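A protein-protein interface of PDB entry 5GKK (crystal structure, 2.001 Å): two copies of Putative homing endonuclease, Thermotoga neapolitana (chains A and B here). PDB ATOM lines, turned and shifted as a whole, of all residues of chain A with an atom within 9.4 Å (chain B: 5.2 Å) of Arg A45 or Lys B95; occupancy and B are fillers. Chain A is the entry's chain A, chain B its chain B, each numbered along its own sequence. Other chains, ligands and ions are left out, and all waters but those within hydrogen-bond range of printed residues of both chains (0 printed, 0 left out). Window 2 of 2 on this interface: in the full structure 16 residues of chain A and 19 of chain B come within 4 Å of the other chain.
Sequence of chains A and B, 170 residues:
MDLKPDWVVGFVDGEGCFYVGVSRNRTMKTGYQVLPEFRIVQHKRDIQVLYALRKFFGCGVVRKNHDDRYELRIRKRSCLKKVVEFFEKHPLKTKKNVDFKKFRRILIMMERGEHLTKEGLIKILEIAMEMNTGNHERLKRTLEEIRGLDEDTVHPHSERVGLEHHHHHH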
ATOM      1  N   MET A   1       0.279 -32.956  15.668  1.00  0.00           N
ATOM      2  CA  MET A   1       0.233 -32.483  14.289  1.00  0.00           C
ATOM      3  C   MET A   1       0.512 -33.631  13.312  1.00  0.00           C
ATOM      4  O   MET A   1       1.157 -34.615  13.676  1.00  0.00           O
ATOM      5  CB  MET A   1       1.253 -31.366  14.086  1.00  0.00           C
ATOM      6  CG  MET A   1       2.647 -31.758  14.510  1.00  0.00           C
ATOM      7  SD  MET A   1       3.870 -30.546  13.983  1.00  0.00           S
ATOM      8  CE  MET A   1       5.222 -30.858  15.076  1.00  0.00           C
ATOM      9  N   TRP A   7       8.164 -34.065   3.997  1.00  0.00           N
ATOM     10  CA  TRP A   7       8.627 -33.273   5.129  1.00  0.00           C
ATOM     11  C   TRP A   7       9.444 -34.147   6.076  1.00  0.00           C
ATOM     12  O   TRP A   7      10.491 -33.734   6.593  1.00  0.00           O
ATOM     13  CB  TRP A   7       7.450 -32.643   5.892  1.00  0.00           C
ATOM     14  CG  TRP A   7       7.892 -31.732   7.026  1.00  0.00           C
ATOM     15  CD1 TRP A   7       7.977 -30.372   6.993  1.00  0.00           C
ATOM     16  CD2 TRP A   7       8.295 -32.128   8.358  1.00  0.00           C
ATOM     17  NE1 TRP A   7       8.427 -29.891   8.222  1.00  0.00           N
ATOM     18  CE2 TRP A   7       8.632 -30.949   9.063  1.00  0.00           C
ATOM     19  CE3 TRP A   7       8.449 -33.367   9.001  1.00  0.00           C
ATOM     20  CZ2 TRP A   7       9.083 -30.978  10.383  1.00  0.00           C
ATOM     21  CZ3 TRP A   7       8.894 -33.393  10.307  1.00  0.00           C
ATOM     22  CH2 TRP A   7       9.203 -32.206  10.989  1.00  0.00           C
ATOM     23  N   PHE A  11      13.314 -33.450   7.141  1.00  0.00           N
ATOM     24  CA  PHE A  11      13.681 -33.353   8.546  1.00  0.00           C
ATOM     25  C   PHE A  11      14.704 -34.429   8.963  1.00  0.00           C
ATOM     26  O   PHE A  11      15.672 -34.140   9.679  1.00  0.00           O
ATOM     27  CB  PHE A  11      12.423 -33.435   9.418  1.00  0.00           C
ATOM     28  CG  PHE A  11      12.637 -32.971  10.846  1.00  0.00           C
ATOM     29  CD1 PHE A  11      12.770 -31.615  11.140  1.00  0.00           C
ATOM     30  CD2 PHE A  11      12.694 -33.882  11.878  1.00  0.00           C
ATOM     31  CE1 PHE A  11      12.957 -31.182  12.432  1.00  0.00           C
ATOM     32  CE2 PHE A  11      12.873 -33.460  13.188  1.00  0.00           C
ATOM     33  CZ  PHE A  11      13.008 -32.108  13.461  1.00  0.00           C
ATOM     34  N   GLN A  42      15.935 -33.295  19.768  1.00  0.00           N
ATOM     35  CA  GLN A  42      15.424 -31.932  19.638  1.00  0.00           C
ATOM     36  C   GLN A  42      15.491 -31.228  20.970  1.00  0.00           C
ATOM     37  O   GLN A  42      15.500 -31.871  22.027  1.00  0.00           O
ATOM     38  CB  GLN A  42      13.975 -31.927  19.143  1.00  0.00           C
ATOM     39  CG  GLN A  42      13.805 -32.173  17.620  1.00  0.00           C
ATOM     40  CD  GLN A  42      14.367 -31.038  16.768  1.00  0.00           C
ATOM     41  OE1 GLN A  42      13.706 -30.049  16.549  1.00  0.00           O
ATOM     42  NE2 GLN A  42      15.580 -31.195  16.283  1.00  0.00           N
ATOM     43  N   HIS A  43      15.549 -29.903  20.918  1.00  0.00           N
ATOM     44  CA  HIS A  43      15.407 -29.110  22.132  1.00  0.00           C
ATOM     45  C   HIS A  43      13.983 -29.275  22.660  1.00  0.00           C
ATOM     46  O   HIS A  43      13.027 -29.452  21.891  1.00  0.00           O
ATOM     47  CB  HIS A  43      15.723 -27.632  21.862  1.00  0.00           C
ATOM     48  CG  HIS A  43      15.765 -26.794  23.108  1.00  0.00           C
ATOM     49  ND1 HIS A  43      14.634 -26.297  23.715  1.00  0.00           N
ATOM     50  CD2 HIS A  43      16.812 -26.391  23.873  1.00  0.00           C
ATOM     51  CE1 HIS A  43      14.978 -25.619  24.800  1.00  0.00           C
ATOM     52  NE2 HIS A  43      16.291 -25.661  24.913  1.00  0.00           N
ATOM     53  N   LYS A  44      13.827 -29.190  23.977  1.00  0.00           N
ATOM     54  CA  LYS A  44      12.539 -29.438  24.617  1.00  0.00           C
ATOM     55  C   LYS A  44      11.376 -28.591  24.088  1.00  0.00           C
ATOM     56  O   LYS A  44      10.221 -29.018  24.130  1.00  0.00           O
ATOM     57  CB  LYS A  44      12.665 -29.269  26.128  1.00  0.00           C
ATOM     58  CG  LYS A  44      12.876 -27.817  26.566  1.00  0.00           C
ATOM     59  CD  LYS A  44      12.935 -27.689  28.080  1.00  0.00           C
ATOM     60  CE  LYS A  44      12.760 -26.239  28.511  1.00  0.00           C
ATOM     61  NZ  LYS A  44      13.765 -25.329  27.863  1.00  0.00           N
ATOM     62  N   ARG A  45      11.652 -27.402  23.575  1.00  0.00           N
ATOM     63  CA  ARG A  45      10.565 -26.568  23.045  1.00  0.00           C
ATOM     64  C   ARG A  45       9.935 -27.203  21.804  1.00  0.00           C
ATOM     65  O   ARG A  45       8.836 -26.816  21.362  1.00  0.00           O
ATOM     66  CB  ARG A  45      11.086 -25.189  22.666  1.00  0.00           C
ATOM     67  CG  ARG A  45      12.059 -25.224  21.496  1.00  0.00           C
ATOM     68  CD  ARG A  45      12.434 -23.812  21.106  1.00  0.00           C
ATOM     69  NE  ARG A  45      13.370 -23.246  22.062  1.00  0.00           N
ATOM     70  CZ  ARG A  45      14.689 -23.380  21.948  1.00  0.00           C
ATOM     71  NH1 ARG A  45      15.197 -24.049  20.912  1.00  0.00           N
ATOM     72  NH2 ARG A  45      15.501 -22.849  22.858  1.00  0.00           N
ATOM     73  N   ASP A  46      10.645 -28.169  21.227  1.00  0.00           N
ATOM     74  CA  ASP A  46      10.164 -28.815  20.027  1.00  0.00           C
ATOM     75  C   ASP A  46       9.800 -30.264  20.307  1.00  0.00           C
ATOM     76  O   ASP A  46       9.861 -31.105  19.390  1.00  0.00           O
ATOM     77  CB  ASP A  46      11.221 -28.744  18.909  1.00  0.00           C
ATOM     78  CG  ASP A  46      11.074 -27.494  18.056  1.00  0.00           C
ATOM     79  OD1 ASP A  46       9.929 -27.186  17.668  1.00  0.00           O
ATOM     80  OD2 ASP A  46      12.089 -26.813  17.785  1.00  0.00           O
ATOM     81  N   ILE A  47       9.343 -30.501  21.506  1.00  0.00           N
ATOM     82  CA  ILE A  47       8.944 -31.802  21.930  1.00  0.00           C
ATOM     83  C   ILE A  47       7.808 -32.267  21.016  1.00  0.00           C
ATOM     84  O   ILE A  47       7.726 -33.422  20.653  1.00  0.00           O
ATOM     85  CB  ILE A  47       8.606 -31.734  23.441  1.00  0.00           C
ATOM     86  CG1 ILE A  47       9.405 -32.772  24.200  1.00  0.00           C
ATOM     87  CG2 ILE A  47       7.122 -31.797  23.739  1.00  0.00           C
ATOM     88  CD1 ILE A  47       8.822 -34.144  24.089  1.00  0.00           C
ATOM     89  N   GLN A  48       6.937 -31.357  20.637  1.00  0.00           N
ATOM     90  CA  GLN A  48       5.765 -31.741  19.848  1.00  0.00           C
ATOM     91  C   GLN A  48       6.165 -32.461  18.526  1.00  0.00           C
ATOM     92  O   GLN A  48       5.493 -33.395  18.080  1.00  0.00           O
ATOM     93  CB  GLN A  48       4.831 -30.558  19.558  1.00  0.00           C
ATOM     94  CG  GLN A  48       3.677 -30.954  18.607  1.00  0.00           C
ATOM     95  CD  GLN A  48       2.615 -29.880  18.430  1.00  0.00           C
ATOM     96  OE1 GLN A  48       2.878 -28.690  18.594  1.00  0.00           O
ATOM     97  NE2 GLN A  48       1.411 -30.302  18.073  1.00  0.00           N
ATOM     98  N   VAL A  49       7.259 -32.024  17.917  1.00  0.00           N
ATOM     99  CA  VAL A  49       7.703 -32.622  16.658  1.00  0.00           C
ATOM    100  C   VAL A  49       8.092 -34.087  16.841  1.00  0.00           C
ATOM    101  O   VAL A  49       7.853 -34.919  15.956  1.00  0.00           O
ATOM    102  CB  VAL A  49       8.879 -31.849  16.025  1.00  0.00           C
ATOM    103  CG1 VAL A  49       8.958 -32.163  14.546  1.00  0.00           C
ATOM    104  CG2 VAL A  49       8.656 -30.369  16.184  1.00  0.00           C
ATOM    105  N   LEU A  50       8.671 -34.394  17.994  1.00  0.00           N
ATOM    106  CA  LEU A  50       9.091 -35.759  18.309  1.00  0.00           C
ATOM    107  C   LEU A  50       7.871 -36.657  18.410  1.00  0.00           C
ATOM    108  O   LEU A  50       7.869 -37.765  17.886  1.00  0.00           O
ATOM    109  CB  LEU A  50       9.903 -35.812  19.595  1.00  0.00           C
ATOM    110  CG  LEU A  50      11.232 -35.057  19.604  1.00  0.00           C
ATOM    111  CD1 LEU A  50      11.960 -35.150  20.981  1.00  0.00           C
ATOM    112  CD2 LEU A  50      12.137 -35.557  18.489  1.00  0.00           C
ATOM    113  N   ASP A  68      18.651 -30.093  28.400  1.00  0.00           N
ATOM    114  CA  ASP A  68      17.375 -29.597  27.872  1.00  0.00           C
ATOM    115  C   ASP A  68      16.931 -30.288  26.583  1.00  0.00           C
ATOM    116  O   ASP A  68      16.101 -29.757  25.856  1.00  0.00           O
ATOM    117  CB  ASP A  68      17.431 -28.068  27.636  1.00  0.00           C
ATOM    118  CG  ASP A  68      18.689 -27.612  26.871  1.00  0.00           C
ATOM    119  OD1 ASP A  68      18.958 -26.393  26.894  1.00  0.00           O
ATOM    120  OD2 ASP A  68      19.395 -28.455  26.271  1.00  0.00           O
ATOM    121  N   ARG A  69      17.462 -31.475  26.311  1.00  0.00           N
ATOM    122  CA  ARG A  69      17.130 -32.170  25.069  1.00  0.00           C
ATOM    123  C   ARG A  69      16.311 -33.449  25.250  1.00  0.00           C
ATOM    124  O   ARG A  69      16.403 -34.125  26.281  1.00  0.00           O
ATOM    125  CB  ARG A  69      18.402 -32.526  24.296  1.00  0.00           C
ATOM    126  CG  ARG A  69      19.231 -31.350  23.813  1.00  0.00           C
ATOM    127  CD  ARG A  69      20.637 -31.867  23.504  1.00  0.00           C
ATOM    128  NE  ARG A  69      21.554 -30.838  23.026  1.00  0.00           N
ATOM    129  CZ  ARG A  69      22.871 -31.012  22.951  1.00  0.00           C
ATOM    130  NH1 ARG A  69      23.406 -32.166  23.338  1.00  0.00           N
ATOM    131  NH2 ARG A  69      23.653 -30.040  22.497  1.00  0.00           N
ATOM    132  N   TYR A  70      15.525 -33.779  24.220  1.00  0.00           N
ATOM    133  CA  TYR A  70      14.690 -34.974  24.215  1.00  0.00           C
ATOM    134  C   TYR A  70      14.902 -35.740  22.910  1.00  0.00           C
ATOM    135  O   TYR A  70      15.391 -35.177  21.943  1.00  0.00           O
ATOM    136  CB  TYR A  70      13.214 -34.594  24.379  1.00  0.00           C
ATOM    137  CG  TYR A  70      12.868 -34.162  25.787  1.00  0.00           C
ATOM    138  CD1 TYR A  70      12.227 -35.030  26.664  1.00  0.00           C
ATOM    139  CD2 TYR A  70      13.233 -32.901  26.255  1.00  0.00           C
ATOM    140  CE1 TYR A  70      11.943 -34.640  27.983  1.00  0.00           C
ATOM    141  CE2 TYR A  70      12.939 -32.506  27.550  1.00  0.00           C
ATOM    142  CZ  TYR A  70      12.297 -33.380  28.409  1.00  0.00           C
ATOM    143  OH  TYR A  70      12.003 -32.982  29.702  1.00  0.00           O
ATOM    144  N   LYS B  93       7.103 -26.250  10.580  1.00  0.00           N
ATOM    145  CA  LYS B  93       6.317 -27.115  11.448  1.00  0.00           C
ATOM    146  C   LYS B  93       6.764 -27.038  12.910  1.00  0.00           C
ATOM    147  O   LYS B  93       5.982 -27.307  13.800  1.00  0.00           O
ATOM    148  CB  LYS B  93       6.432 -28.572  10.962  1.00  0.00           C
ATOM    149  CG  LYS B  93       5.127 -29.228  10.614  1.00  0.00           C
ATOM    150  CD  LYS B  93       4.338 -28.392   9.616  1.00  0.00           C
ATOM    151  CE  LYS B  93       2.961 -28.981   9.384  1.00  0.00           C
ATOM    152  NZ  LYS B  93       2.840 -29.555   8.011  1.00  0.00           N
ATOM    153  N   THR B  94       8.039 -26.725  13.131  1.00  0.00           N
ATOM    154  CA  THR B  94       8.618 -26.672  14.456  1.00  0.00           C
ATOM    155  C   THR B  94       8.448 -25.264  15.003  1.00  0.00           C
ATOM    156  O   THR B  94       7.704 -24.465  14.427  1.00  0.00           O
ATOM    157  CB  THR B  94      10.132 -27.041  14.445  1.00  0.00           C
ATOM    158  OG1 THR B  94      10.880 -26.051  13.731  1.00  0.00           O
ATOM    159  CG2 THR B  94      10.367 -28.421  13.794  1.00  0.00           C
ATOM    160  N   LYS B  95       9.155 -24.965  16.093  1.00  0.00           N
ATOM    161  CA  LYS B  95       9.178 -23.621  16.659  1.00  0.00           C
ATOM    162  C   LYS B  95       9.897 -22.622  15.761  1.00  0.00           C
ATOM    163  O   LYS B  95       9.765 -21.414  15.961  1.00  0.00           O
ATOM    164  CB  LYS B  95       9.854 -23.609  18.038  1.00  0.00           C
ATOM    165  CG  LYS B  95       8.993 -24.114  19.179  1.00  0.00           C
ATOM    166  CD  LYS B  95       7.536 -23.737  18.991  1.00  0.00           C
ATOM    167  CE  LYS B  95       6.711 -24.047  20.235  1.00  0.00           C
ATOM    168  NZ  LYS B  95       7.112 -23.154  21.365  1.00  0.00           N
ATOM    169  N   LYS B  96      10.673 -23.110  14.792  1.00  0.00           N
ATOM    170  CA  LYS B  96      11.230 -22.214  13.781  1.00  0.00           C
ATOM    171  C   LYS B  96      10.130 -21.357  13.127  1.00  0.00           C
ATOM    172  O   LYS B  96      10.414 -20.280  12.617  1.00  0.00           O
ATOM    173  CB  LYS B  96      11.965 -22.980  12.683  1.00  0.00           C
ATOM    174  CG  LYS B  96      13.051 -23.927  13.153  1.00  0.00           C
ATOM    175  CD  LYS B  96      14.397 -23.278  13.140  1.00  0.00           C
ATOM    176  CE  LYS B  96      15.432 -24.217  13.704  1.00  0.00           C
ATOM    177  NZ  LYS B  96      16.021 -25.029  12.645  1.00  0.00           N
ATOM    178  N   ASN B  97       8.885 -21.838  13.133  1.00  0.00           N
ATOM    179  CA  ASN B  97       7.762 -21.061  12.587  1.00  0.00           C
ATOM    180  C   ASN B  97       7.591 -19.732  13.340  1.00  0.00           C
ATOM    181  O   ASN B  97       7.254 -18.700  12.746  1.00  0.00           O
ATOM    182  CB  ASN B  97       6.453 -21.863  12.632  1.00  0.00           C
ATOM    183  CG  ASN B  97       5.410 -21.365  11.624  1.00  0.00           C
ATOM    184  OD1 ASN B  97       5.735 -20.704  10.643  1.00  0.00           O
ATOM    185  ND2 ASN B  97       4.152 -21.710  11.860  1.00  0.00           N
ATOM    186  N   VAL B  98       7.851 -19.766  14.643  1.00  0.00           N
ATOM    187  CA  VAL B  98       7.697 -18.582  15.473  1.00  0.00           C
ATOM    188  C   VAL B  98       8.848 -17.593  15.231  1.00  0.00           C
ATOM    189  O   VAL B  98       8.609 -16.407  15.057  1.00  0.00           O
ATOM    190  CB  VAL B  98       7.535 -18.935  16.962  1.00  0.00           C
ATOM    191  CG1 VAL B  98       7.220 -17.688  17.762  1.00  0.00           C
ATOM    192  CG2 VAL B  98       6.418 -19.940  17.147  1.00  0.00           C
ATOM    193  N   ASP B  99      10.085 -18.087  15.194  1.00  0.00           N
ATOM    194  CA  ASP B  99      11.226 -17.286  14.752  1.00  0.00           C
ATOM    195  C   ASP B  99      10.966 -16.734  13.343  1.00  0.00           C
ATOM    196  O   ASP B  99      11.317 -15.594  13.024  1.00  0.00           O
ATOM    197  CB  ASP B  99      12.513 -18.130  14.699  1.00  0.00           C
ATOM    198  CG  ASP B  99      13.115 -18.408  16.071  1.00  0.00           C
ATOM    199  OD1 ASP B  99      12.618 -17.866  17.076  1.00  0.00           O
ATOM    200  OD2 ASP B  99      14.113 -19.164  16.134  1.00  0.00           O
ATOM    201  N   ASN B 132      14.248 -17.102  19.320  1.00  0.00           N
ATOM    202  CA  ASN B 132      15.097 -18.086  19.981  1.00  0.00           C
ATOM    203  C   ASN B 132      16.565 -18.009  19.578  1.00  0.00           C
ATOM    204  O   ASN B 132      17.444 -18.445  20.322  1.00  0.00           O
ATOM    205  CB  ASN B 132      14.557 -19.490  19.726  1.00  0.00           C
ATOM    206  CG  ASN B 132      13.329 -19.786  20.544  1.00  0.00           C
ATOM    207  OD1 ASN B 132      13.358 -19.654  21.764  1.00  0.00           O
ATOM    208  ND2 ASN B 132      12.230 -20.163  19.882  1.00  0.00           N
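No position is printed for both chains.
Of the 7 pairs that touch across the chains among the printed residues, none has its exchanged pair printed and touching as well.
The side-chain carboxylate (OD1) of Asp A46 lies within hydrogen-bond range of the backbone NH (N) of Lys B95 (2.8 Å).
Of chain B, only Lys B95 (3.5 Å) and Asn B132 (3.6 Å) come within 4 Å of Arg A45.
Printed residues of chain A within 4 Å of Lys B95: Arg A45 (3.5 Å) and Asp A46 (2.8 Å).
Of chain A, only Asp A46 and Val A49 come within 4 Å of Thr B94.
Val B98 touches none of the printed residues of chain A.
Of the printed residues of chain B, Asp A46 touches Thr B94 (3.2 Å) and Lys B95 (2.8 Å).
Of the printed residues of chain A, Lys B93 touches Met A1 and Trp A7.
Of the printed residues of chain B, Val A49 touches Thr B94 (3.5 Å).
Printed residues of chain B within 4 Å of Trp A7: Lys B93 (3.6 Å).
Printed residues of chain A within 4 Å of Asn B132: Arg A45.
Tyr A70 touches none of the printed residues of chain B.
Gln A42 touches none of the printed residues of chain B.
The nearest printed residue of chain B that does not touch Arg A45 is Thr B94 (6.6 Å).
The nearest residue of chain A that does not touch Lys B95 is Val A49 (5.4 Å).
Printed residues of chain A that touch a printed residue of chain B: Met A1, Trp A7, Arg A45, Asp A46 and Val A49.
Hydrophobic or aromatic side chains of chain A that line the printed part of chain B: Met A1, Trp A7 and Val A49.
Of the 8 printed residues of chain B, 4 touch a printed residue of chain A.
Among the printed residues, 7 pairs touch across the chains.
Among the printed residues, no Asp or Glu carboxylate lies within 4 Å of a Lys or Arg side-chain nitrogen of the other chain.
Among the printed residues, pairs that only touch across the chains: Met A1 with Lys B93 (3.8 Å), Trp A7 with Lys B93 (3.6 Å), Arg A45 with Lys B95 (3.5 Å), Arg A45 with Asn B132 (3.6 Å), Asp A46 with Thr B94 (3.2 Å) and Val A49 with Thr B94 (3.5 Å).
The side-chain carboxylate (OD1) of Asp B99 lies within hydrogen-bond range of the backbone NH (N) of Asn B132, 2.9 Å away.
The backbone NH (N) of Lys B96 lies close to the side-chain hydroxyl (OG1) of Thr B94 (3.1 Å).
ND1 of His A43 lies close to N of Arg A45, at 3.2 Å.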
